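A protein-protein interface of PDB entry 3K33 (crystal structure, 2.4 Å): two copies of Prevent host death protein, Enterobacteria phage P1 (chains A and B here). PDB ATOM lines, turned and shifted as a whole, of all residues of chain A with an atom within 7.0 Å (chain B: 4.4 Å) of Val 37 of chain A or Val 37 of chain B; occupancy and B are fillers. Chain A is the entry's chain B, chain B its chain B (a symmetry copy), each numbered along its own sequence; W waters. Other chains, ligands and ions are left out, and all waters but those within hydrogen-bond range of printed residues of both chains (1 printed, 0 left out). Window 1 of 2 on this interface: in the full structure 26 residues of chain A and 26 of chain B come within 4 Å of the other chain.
Hydrophobic or aromatic side chains of chain A that line the printed part of chain B: Met 1, Leu 17, Val 20, Pro 35, Ala 36, Val 37, Ile 38, Val 39 and Phe 44.
Printed residues of chain B that touch a printed residue of chain A: Met 1, Glu 27, Ala 36, Val 37, Ile 38, Val 39, Lys 41 and Phe 44.
Among the printed residues, 26 pairs touch across the chains.
Of the printed residues of chain B, Ala 36 of chain A touches Ile 38 (3.95 Å), Val 39 (3.4 Å) and Lys 41 (3.8 Å).
Of the printed residues of chain B, Val 37 of chain A touches Val 37 (3.4 Å), Ile 38 (3.2 Å), Val 39 (2.7 Å), Lys 41 (3.8 Å) and Phe 44 (3.99 Å).
Of the printed residues of chain B, Lys 41 of chain A touches Met 1, Glu 27, Ala 36 and Val 37.
Of the printed residues of chain A, Met 1 of chain B touches Lys 41 (3.2 Å) and Glu 45 (3.3 Å).
Of the printed residues of chain A, Ala 36 of chain B touches Leu 17 (3.4 Å), Val 20 (3.996 Å), Ile 38 (3.95 Å), Val 39 (3.4 Å) and Lys 41 (3.8 Å).
Printed residues of chain A within 4 Å of Lys 41 of chain B: Met 1 (3.2 Å), Glu 27 (3.0 Å), Pro 35 (3.0 Å), Ala 36 (3.8 Å) and Val 37 (3.8 Å).
The nearest printed residue of chain B that does not touch Glu 45 of chain A is Val 37 of chain B (5.0 Å).
Phe 44 of chain B touches Glu 25 of chain A (CZ to OE2, 3.4 Å).
Ala 36 of chain A touches Ile 38 of chain B.
CA of Ala 36 of chain A touches O of Val 39 of chain B (3.4 Å).
Ile 38 of chain B touches Val 37 of chain A (CA to O, 3.2 Å).
CG1 of Ile 38 of chain A touches CB of Ala 36 of chain B, 3.95 Å away.
CE1 of Phe 44 of chain B touches CG1 of Val 39 of chain A, 3.8 Å away.
CE of Lys 41 of chain A touches OE1 of Glu 27 of chain B, at 3.0 Å.
Lys 41 of chain A touches Ala 36 of chain B.
Val 37 of chain B touches Lys 41 of chain A (CG2 to CG, 3.8 Å).
Phe 44 of chain A touches Val 39 of chain B (CE1 to CG1, 3.8 Å).
O of Val 26 of chain A lies within hydrogen-bond range of N of Ile 38 of chain A.
N of Ile 28 of chain A lies within hydrogen-bond range of O of Ala 36 of chain A, 2.9 Å away.
The side-chain amino group (NZ) of Lys 41 of chain A is in salt-bridge range of the side-chain carboxylate (OE2) of Glu 45 of chain A (3.1 Å).
The backbone carbonyl oxygen (O) of Val 26 of chain B is in hydrogen-bond range of the backbone NH (N) of Ile 38 of chain B, 2.9 Å away.
Glu 27 of chain A touches Lys 41 of chain B, and with the chains exchanged Lys 41 of chain A touches Glu 27 of chain B.
Ala 36 of chain A touches Lys 41 of chain B, and with the chains exchanged Lys 41 of chain A touches Ala 36 of chain B.
Val 37 of chain A touches Ile 38 of chain B, and with the chains exchanged Ile 38 of chain A touches Val 37 of chain B.
Val 39 of chain A touches Phe 44 of chain B, and with the chains exchanged Phe 44 of chain A touches Val 39 of chain B.
Water W1 bridges the backbone carbonyl oxygen (O) of Pro 35 of chain A (2.9 Å) and the backbone NH (N) of Lys 41 of chain B (3.2 Å).
The backbone carbonyl oxygen of Pro 35 of chain A lies within hydrogen-bond range of the backbone NH of Lys 41 of chain B.
O of Val 39 of chain B sits at hydrogen-bond distance from N of Val 37 of chain A (2.7 Å).
The backbone NH of Val 37 of chain B is in hydrogen-bond range of the backbone carbonyl oxygen of Val 39 of chain A.
The backbone carbonyl oxygen (O) of Val 37 of chain B lies close to the backbone carbonyl oxygen (O) of Val 37 of chain A (3.4 Å).
The side-chain sulfur (SD) of Met 1 of chain B sits close to the side-chain carboxylate (OE2) of Glu 45 of chain A (3.7 Å).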
ATOM      1  N   MET A   1     -32.762  18.952 -23.757  1.00  0.00           N
ATOM      2  CA  MET A   1     -31.493  19.082 -22.984  1.00  0.00           C
ATOM      3  C   MET A   1     -30.340  19.557 -23.861  1.00  0.00           C
ATOM      4  O   MET A   1     -29.721  18.770 -24.580  1.00  0.00           O
ATOM      5  CB  MET A   1     -31.117  17.751 -22.318  1.00  0.00           C
ATOM      6  CG  MET A   1     -29.870  17.824 -21.426  1.00  0.00           C
ATOM      7  SD  MET A   1     -29.549  16.309 -20.493  1.00  0.00           S
ATOM      8  CE  MET A   1     -29.241  15.170 -21.826  1.00  0.00           C
ATOM      9  N   LEU A  17     -28.328  28.756 -14.510  1.00  0.00           N
ATOM     10  CA  LEU A  17     -29.273  28.583 -13.420  1.00  0.00           C
ATOM     11  C   LEU A  17     -30.622  29.236 -13.713  1.00  0.00           C
ATOM     12  O   LEU A  17     -31.644  28.725 -13.277  1.00  0.00           O
ATOM     13  CB  LEU A  17     -28.674  29.107 -12.105  1.00  0.00           C
ATOM     14  CG  LEU A  17     -27.528  28.250 -11.540  1.00  0.00           C
ATOM     15  CD1 LEU A  17     -26.723  29.022 -10.537  1.00  0.00           C
ATOM     16  CD2 LEU A  17     -28.065  26.983 -10.894  1.00  0.00           C
ATOM     17  N   VAL A  20     -32.305  26.924 -16.081  1.00  0.00           N
ATOM     18  CA  VAL A  20     -32.593  25.758 -15.261  1.00  0.00           C
ATOM     19  C   VAL A  20     -33.830  26.009 -14.405  1.00  0.00           C
ATOM     20  O   VAL A  20     -34.695  25.153 -14.297  1.00  0.00           O
ATOM     21  CB  VAL A  20     -31.350  25.412 -14.390  1.00  0.00           C
ATOM     22  CG1 VAL A  20     -31.734  24.575 -13.189  1.00  0.00           C
ATOM     23  CG2 VAL A  20     -30.310  24.713 -15.256  1.00  0.00           C
ATOM     24  N   GLU A  24     -35.236  24.101 -17.755  1.00  0.00           N
ATOM     25  CA  GLU A  24     -34.320  23.422 -18.660  1.00  0.00           C
ATOM     26  C   GLU A  24     -33.351  22.474 -17.952  1.00  0.00           C
ATOM     27  O   GLU A  24     -33.005  22.664 -16.781  1.00  0.00           O
ATOM     28  CB  GLU A  24     -33.568  24.451 -19.497  1.00  0.00           C
ATOM     29  CG  GLU A  24     -32.435  23.895 -20.351  1.00  0.00           C
ATOM     30  CD  GLU A  24     -31.795  24.956 -21.235  1.00  0.00           C
ATOM     31  OE1 GLU A  24     -31.719  26.126 -20.802  1.00  0.00           O
ATOM     32  OE2 GLU A  24     -31.348  24.616 -22.354  1.00  0.00           O
ATOM     33  N   GLU A  25     -32.944  21.436 -18.678  1.00  0.00           N
ATOM     34  CA  GLU A  25     -31.959  20.470 -18.205  1.00  0.00           C
ATOM     35  C   GLU A  25     -30.708  20.759 -19.024  1.00  0.00           C
ATOM     36  O   GLU A  25     -30.737  20.750 -20.254  1.00  0.00           O
ATOM     37  CB  GLU A  25     -32.474  19.047 -18.433  1.00  0.00           C
ATOM     38  CG  GLU A  25     -33.937  18.877 -17.984  1.00  0.00           C
ATOM     39  CD  GLU A  25     -34.506  17.471 -18.181  1.00  0.00           C
ATOM     40  OE1 GLU A  25     -34.031  16.726 -19.061  1.00  0.00           O
ATOM     41  OE2 GLU A  25     -35.468  17.125 -17.462  1.00  0.00           O
ATOM     42  N   VAL A  26     -29.615  21.064 -18.339  1.00  0.00           N
ATOM     43  CA  VAL A  26     -28.386  21.432 -19.028  1.00  0.00           C
ATOM     44  C   VAL A  26     -27.241  20.496 -18.670  1.00  0.00           C
ATOM     45  O   VAL A  26     -26.860  20.364 -17.507  1.00  0.00           O
ATOM     46  CB  VAL A  26     -27.960  22.887 -18.719  1.00  0.00           C
ATOM     47  CG1 VAL A  26     -26.733  23.265 -19.540  1.00  0.00           C
ATOM     48  CG2 VAL A  26     -29.089  23.843 -19.001  1.00  0.00           C
ATOM     49  N   GLU A  27     -26.704  19.853 -19.692  1.00  0.00           N
ATOM     50  CA  GLU A  27     -25.584  18.956 -19.538  1.00  0.00           C
ATOM     51  C   GLU A  27     -24.327  19.802 -19.570  1.00  0.00           C
ATOM     52  O   GLU A  27     -24.232  20.750 -20.361  1.00  0.00           O
ATOM     53  CB  GLU A  27     -25.547  17.966 -20.701  1.00  0.00           C
ATOM     54  CG  GLU A  27     -24.475  16.890 -20.570  1.00  0.00           C
ATOM     55  CD  GLU A  27     -24.329  16.070 -21.829  1.00  0.00           C
ATOM     56  OE1 GLU A  27     -25.322  15.933 -22.577  1.00  0.00           O
ATOM     57  OE2 GLU A  27     -23.226  15.551 -22.063  1.00  0.00           O
ATOM     58  N   ILE A  28     -23.392  19.481 -18.685  1.00  0.00           N
ATOM     59  CA  ILE A  28     -22.094  20.130 -18.662  1.00  0.00           C
ATOM     60  C   ILE A  28     -21.041  19.051 -18.924  1.00  0.00           C
ATOM     61  O   ILE A  28     -20.920  18.094 -18.167  1.00  0.00           O
ATOM     62  CB  ILE A  28     -21.809  20.825 -17.320  1.00  0.00           C
ATOM     63  CG1 ILE A  28     -22.883  21.876 -17.026  1.00  0.00           C
ATOM     64  CG2 ILE A  28     -20.426  21.476 -17.335  1.00  0.00           C
ATOM     65  CD1 ILE A  28     -22.810  22.421 -15.620  1.00  0.00           C
ATOM     66  N   PRO A  35     -19.932  13.524 -18.068  1.00  0.00           N
ATOM     67  CA  PRO A  35     -20.802  14.695 -18.038  1.00  0.00           C
ATOM     68  C   PRO A  35     -21.723  14.774 -16.811  1.00  0.00           C
ATOM     69  O   PRO A  35     -22.102  13.760 -16.230  1.00  0.00           O
ATOM     70  CB  PRO A  35     -21.590  14.559 -19.340  1.00  0.00           C
ATOM     71  CG  PRO A  35     -21.674  13.113 -19.545  1.00  0.00           C
ATOM     72  CD  PRO A  35     -20.262  12.660 -19.214  1.00  0.00           C
ATOM     73  N   ALA A  36     -22.041  16.001 -16.415  1.00  0.00           N
ATOM     74  CA  ALA A  36     -22.936  16.254 -15.299  1.00  0.00           C
ATOM     75  C   ALA A  36     -24.182  16.881 -15.878  1.00  0.00           C
ATOM     76  O   ALA A  36     -24.247  17.170 -17.076  1.00  0.00           O
ATOM     77  CB  ALA A  36     -22.286  17.199 -14.284  1.00  0.00           C
ATOM     78  N   VAL A  37     -25.185  17.053 -15.036  1.00  0.00           N
ATOM     79  CA  VAL A  37     -26.405  17.734 -15.434  1.00  0.00           C
ATOM     80  C   VAL A  37     -26.830  18.654 -14.315  1.00  0.00           C
ATOM     81  O   VAL A  37     -26.743  18.311 -13.133  1.00  0.00           O
ATOM     82  CB  VAL A  37     -27.561  16.734 -15.765  1.00  0.00           C
ATOM     83  CG1 VAL A  37     -28.927  17.444 -15.758  1.00  0.00           C
ATOM     84  CG2 VAL A  37     -27.340  16.114 -17.135  1.00  0.00           C
ATOM     85  N   ILE A  38     -27.293  19.837 -14.696  1.00  0.00           N
ATOM     86  CA  ILE A  38     -27.854  20.758 -13.728  1.00  0.00           C
ATOM     87  C   ILE A  38     -29.337  20.838 -14.013  1.00  0.00           C
ATOM     88  O   ILE A  38     -29.751  21.070 -15.143  1.00  0.00           O
ATOM     89  CB  ILE A  38     -27.225  22.156 -13.837  1.00  0.00           C
ATOM     90  CG1 ILE A  38     -27.868  23.098 -12.812  1.00  0.00           C
ATOM     91  CG2 ILE A  38     -27.358  22.681 -15.267  1.00  0.00           C
ATOM     92  CD1 ILE A  38     -27.426  24.541 -12.938  1.00  0.00           C
ATOM     93  N   VAL A  39     -30.145  20.636 -12.984  1.00  0.00           N
ATOM     94  CA  VAL A  39     -31.588  20.663 -13.162  1.00  0.00           C
ATOM     95  C   VAL A  39     -32.142  21.219 -11.862  1.00  0.00           C
ATOM     96  O   VAL A  39     -31.431  21.228 -10.849  1.00  0.00           O
ATOM     97  CB  VAL A  39     -32.111  19.235 -13.460  1.00  0.00           C
ATOM     98  CG1 VAL A  39     -31.816  18.316 -12.277  1.00  0.00           C
ATOM     99  CG2 VAL A  39     -33.603  19.245 -13.832  1.00  0.00           C
ATOM    100  N   SER A  40     -33.378  21.718 -11.886  1.00  0.00           N
ATOM    101  CA  SER A  40     -33.982  22.260 -10.674  1.00  0.00           C
ATOM    102  C   SER A  40     -34.076  21.179  -9.624  1.00  0.00           C
ATOM    103  O   SER A  40     -34.293  20.008  -9.926  1.00  0.00           O
ATOM    104  CB  SER A  40     -35.372  22.836 -10.948  1.00  0.00           C
ATOM    105  OG  SER A  40     -36.286  21.804 -11.265  1.00  0.00           O
ATOM    106  N   LYS A  41     -33.909  21.572  -8.372  1.00  0.00           N
ATOM    107  CA  LYS A  41     -33.981  20.608  -7.295  1.00  0.00           C
ATOM    108  C   LYS A  41     -35.353  19.929  -7.256  1.00  0.00           C
ATOM    109  O   LYS A  41     -35.434  18.713  -7.071  1.00  0.00           O
ATOM    110  CB  LYS A  41     -33.690  21.294  -5.977  1.00  0.00           C
ATOM    111  CG  LYS A  41     -33.626  20.359  -4.817  1.00  0.00           C
ATOM    112  CD  LYS A  41     -33.298  21.131  -3.568  1.00  0.00           C
ATOM    113  CE  LYS A  41     -32.835  20.204  -2.467  1.00  0.00           C
ATOM    114  NZ  LYS A  41     -33.863  19.211  -2.091  1.00  0.00           N
ATOM    115  N   ALA A  42     -36.422  20.712  -7.428  1.00  0.00           N
ATOM    116  CA  ALA A  42     -37.786  20.157  -7.428  1.00  0.00           C
ATOM    117  C   ALA A  42     -37.963  19.001  -8.420  1.00  0.00           C
ATOM    118  O   ALA A  42     -38.518  17.955  -8.075  1.00  0.00           O
ATOM    119  CB  ALA A  42     -38.814  21.254  -7.707  1.00  0.00           C
ATOM    120  N   PHE A  44     -35.498  17.233  -9.821  1.00  0.00           N
ATOM    121  CA  PHE A  44     -34.595  16.162  -9.394  1.00  0.00           C
ATOM    122  C   PHE A  44     -35.221  15.322  -8.292  1.00  0.00           C
ATOM    123  O   PHE A  44     -35.270  14.099  -8.385  1.00  0.00           O
ATOM    124  CB  PHE A  44     -33.269  16.726  -8.887  1.00  0.00           C
ATOM    125  CG  PHE A  44     -32.318  15.667  -8.435  1.00  0.00           C
ATOM    126  CD1 PHE A  44     -31.653  14.882  -9.366  1.00  0.00           C
ATOM    127  CD2 PHE A  44     -32.133  15.407  -7.078  1.00  0.00           C
ATOM    128  CE1 PHE A  44     -30.804  13.860  -8.952  1.00  0.00           C
ATOM    129  CE2 PHE A  44     -31.285  14.398  -6.666  1.00  0.00           C
ATOM    130  CZ  PHE A  44     -30.631  13.619  -7.600  1.00  0.00           C
ATOM    131  N   GLU A  45     -35.697  15.975  -7.237  1.00  0.00           N
ATOM    132  CA  GLU A  45     -36.326  15.249  -6.142  1.00  0.00           C
ATOM    133  C   GLU A  45     -37.464  14.348  -6.624  1.00  0.00           C
ATOM    134  O   GLU A  45     -37.590  13.213  -6.170  1.00  0.00           O
ATOM    135  CB  GLU A  45     -36.833  16.215  -5.063  1.00  0.00           C
ATOM    136  CG  GLU A  45     -35.746  16.979  -4.292  1.00  0.00           C
ATOM    137  CD  GLU A  45     -34.574  16.113  -3.806  1.00  0.00           C
ATOM    138  OE1 GLU A  45     -34.762  14.910  -3.489  1.00  0.00           O
ATOM    139  OE2 GLU A  45     -33.453  16.659  -3.723  1.00  0.00           O
ATOM    140  N   MET B   1     -26.879  14.505   0.146  1.00  0.00           N
ATOM    141  CA  MET B   1     -26.886  15.745  -0.682  1.00  0.00           C
ATOM    142  C   MET B   1     -26.473  16.970   0.125  1.00  0.00           C
ATOM    143  O   MET B   1     -27.278  17.554   0.853  1.00  0.00           O
ATOM    144  CB  MET B   1     -28.269  15.982  -1.304  1.00  0.00           C
ATOM    145  CG  MET B   1     -28.336  17.191  -2.249  1.00  0.00           C
ATOM    146  SD  MET B   1     -29.909  17.347  -3.126  1.00  0.00           S
ATOM    147  CE  MET B   1     -31.014  17.620  -1.757  1.00  0.00           C
ATOM    148  N   VAL B  26     -25.257  17.571  -5.482  1.00  0.00           N
ATOM    149  CA  VAL B  26     -24.963  18.854  -4.861  1.00  0.00           C
ATOM    150  C   VAL B  26     -26.004  19.904  -5.224  1.00  0.00           C
ATOM    151  O   VAL B  26     -26.215  20.221  -6.394  1.00  0.00           O
ATOM    152  CB  VAL B  26     -23.561  19.383  -5.251  1.00  0.00           C
ATOM    153  CG1 VAL B  26     -23.254  20.672  -4.497  1.00  0.00           C
ATOM    154  CG2 VAL B  26     -22.506  18.349  -4.966  1.00  0.00           C
ATOM    155  N   GLU B  27     -26.647  20.430  -4.196  1.00  0.00           N
ATOM    156  CA  GLU B  27     -27.640  21.467  -4.356  1.00  0.00           C
ATOM    157  C   GLU B  27     -26.899  22.788  -4.413  1.00  0.00           C
ATOM    158  O   GLU B  27     -25.931  22.995  -3.669  1.00  0.00           O
ATOM    159  CB  GLU B  27     -28.581  21.475  -3.153  1.00  0.00           C
ATOM    160  CG  GLU B  27     -29.746  22.449  -3.280  1.00  0.00           C
ATOM    161  CD  GLU B  27     -30.524  22.585  -1.993  1.00  0.00           C
ATOM    162  OE1 GLU B  27     -30.548  21.617  -1.200  1.00  0.00           O
ATOM    163  OE2 GLU B  27     -31.122  23.650  -1.782  1.00  0.00           O
ATOM    164  N   ALA B  36     -31.001  24.620  -7.488  1.00  0.00           N
ATOM    165  CA  ALA B  36     -30.719  23.699  -8.576  1.00  0.00           C
ATOM    166  C   ALA B  36     -29.969  22.534  -7.975  1.00  0.00           C
ATOM    167  O   ALA B  36     -29.628  22.546  -6.790  1.00  0.00           O
ATOM    168  CB  ALA B  36     -29.874  24.378  -9.658  1.00  0.00           C
ATOM    169  N   VAL B  37     -29.749  21.514  -8.783  1.00  0.00           N
ATOM    170  CA  VAL B  37     -28.955  20.371  -8.366  1.00  0.00           C
ATOM    171  C   VAL B  37     -28.048  19.972  -9.507  1.00  0.00           C
ATOM    172  O   VAL B  37     -28.445  19.980 -10.675  1.00  0.00           O
ATOM    173  CB  VAL B  37     -29.841  19.153  -7.945  1.00  0.00           C
ATOM    174  CG1 VAL B  37     -29.021  17.849  -7.928  1.00  0.00           C
ATOM    175  CG2 VAL B  37     -30.422  19.383  -6.559  1.00  0.00           C
ATOM    176  N   ILE B  38     -26.817  19.623  -9.160  1.00  0.00           N
ATOM    177  CA  ILE B  38     -25.893  19.097 -10.143  1.00  0.00           C
ATOM    178  C   ILE B  38     -25.679  17.639  -9.802  1.00  0.00           C
ATOM    179  O   ILE B  38     -25.368  17.295  -8.667  1.00  0.00           O
ATOM    180  CB  ILE B  38     -24.548  19.841 -10.121  1.00  0.00           C
ATOM    181  CG1 ILE B  38     -23.599  19.232 -11.160  1.00  0.00           C
ATOM    182  CG2 ILE B  38     -23.956  19.814  -8.712  1.00  0.00           C
ATOM    183  CD1 ILE B  38     -22.193  19.795 -11.116  1.00  0.00           C
ATOM    184  N   VAL B  39     -25.854  16.772 -10.788  1.00  0.00           N
ATOM    185  CA  VAL B  39     -25.702  15.347 -10.553  1.00  0.00           C
ATOM    186  C   VAL B  39     -25.155  14.783 -11.853  1.00  0.00           C
ATOM    187  O   VAL B  39     -25.246  15.446 -12.893  1.00  0.00           O
ATOM    188  CB  VAL B  39     -27.069  14.723 -10.171  1.00  0.00           C
ATOM    189  CG1 VAL B  39     -28.057  14.891 -11.323  1.00  0.00           C
ATOM    190  CG2 VAL B  39     -26.919  13.255  -9.739  1.00  0.00           C
ATOM    191  N   LYS B  41     -24.799  12.898 -15.280  1.00  0.00           N
ATOM    192  CA  LYS B  41     -25.797  12.701 -16.310  1.00  0.00           C
ATOM    193  C   LYS B  41     -26.360  11.278 -16.263  1.00  0.00           C
ATOM    194  O   LYS B  41     -27.573  11.091 -16.391  1.00  0.00           O
ATOM    195  CB  LYS B  41     -25.191  12.988 -17.667  1.00  0.00           C
ATOM    196  CG  LYS B  41     -26.175  12.926 -18.787  1.00  0.00           C
ATOM    197  CD  LYS B  41     -25.484  13.259 -20.081  1.00  0.00           C
ATOM    198  CE  LYS B  41     -26.489  13.597 -21.158  1.00  0.00           C
ATOM    199  NZ  LYS B  41     -27.409  12.477 -21.448  1.00  0.00           N
ATOM    200  N   PHE B  44     -28.929  11.028 -13.579  1.00  0.00           N
ATOM    201  CA  PHE B  44     -30.087  11.823 -13.994  1.00  0.00           C
ATOM    202  C   PHE B  44     -30.918  11.083 -15.032  1.00  0.00           C
ATOM    203  O   PHE B  44     -32.127  10.940 -14.883  1.00  0.00           O
ATOM    204  CB  PHE B  44     -29.657  13.167 -14.579  1.00  0.00           C
ATOM    205  CG  PHE B  44     -30.808  14.008 -15.022  1.00  0.00           C
ATOM    206  CD1 PHE B  44     -31.606  14.647 -14.085  1.00  0.00           C
ATOM    207  CD2 PHE B  44     -31.137  14.112 -16.373  1.00  0.00           C
ATOM    208  CE1 PHE B  44     -32.711  15.392 -14.488  1.00  0.00           C
ATOM    209  CE2 PHE B  44     -32.229  14.856 -16.774  1.00  0.00           C
ATOM    210  CZ  PHE B  44     -33.020  15.485 -15.834  1.00  0.00           C
HETATM  211  O   HOH W   1     -22.508  10.858 -16.340  1.00  0.00           O
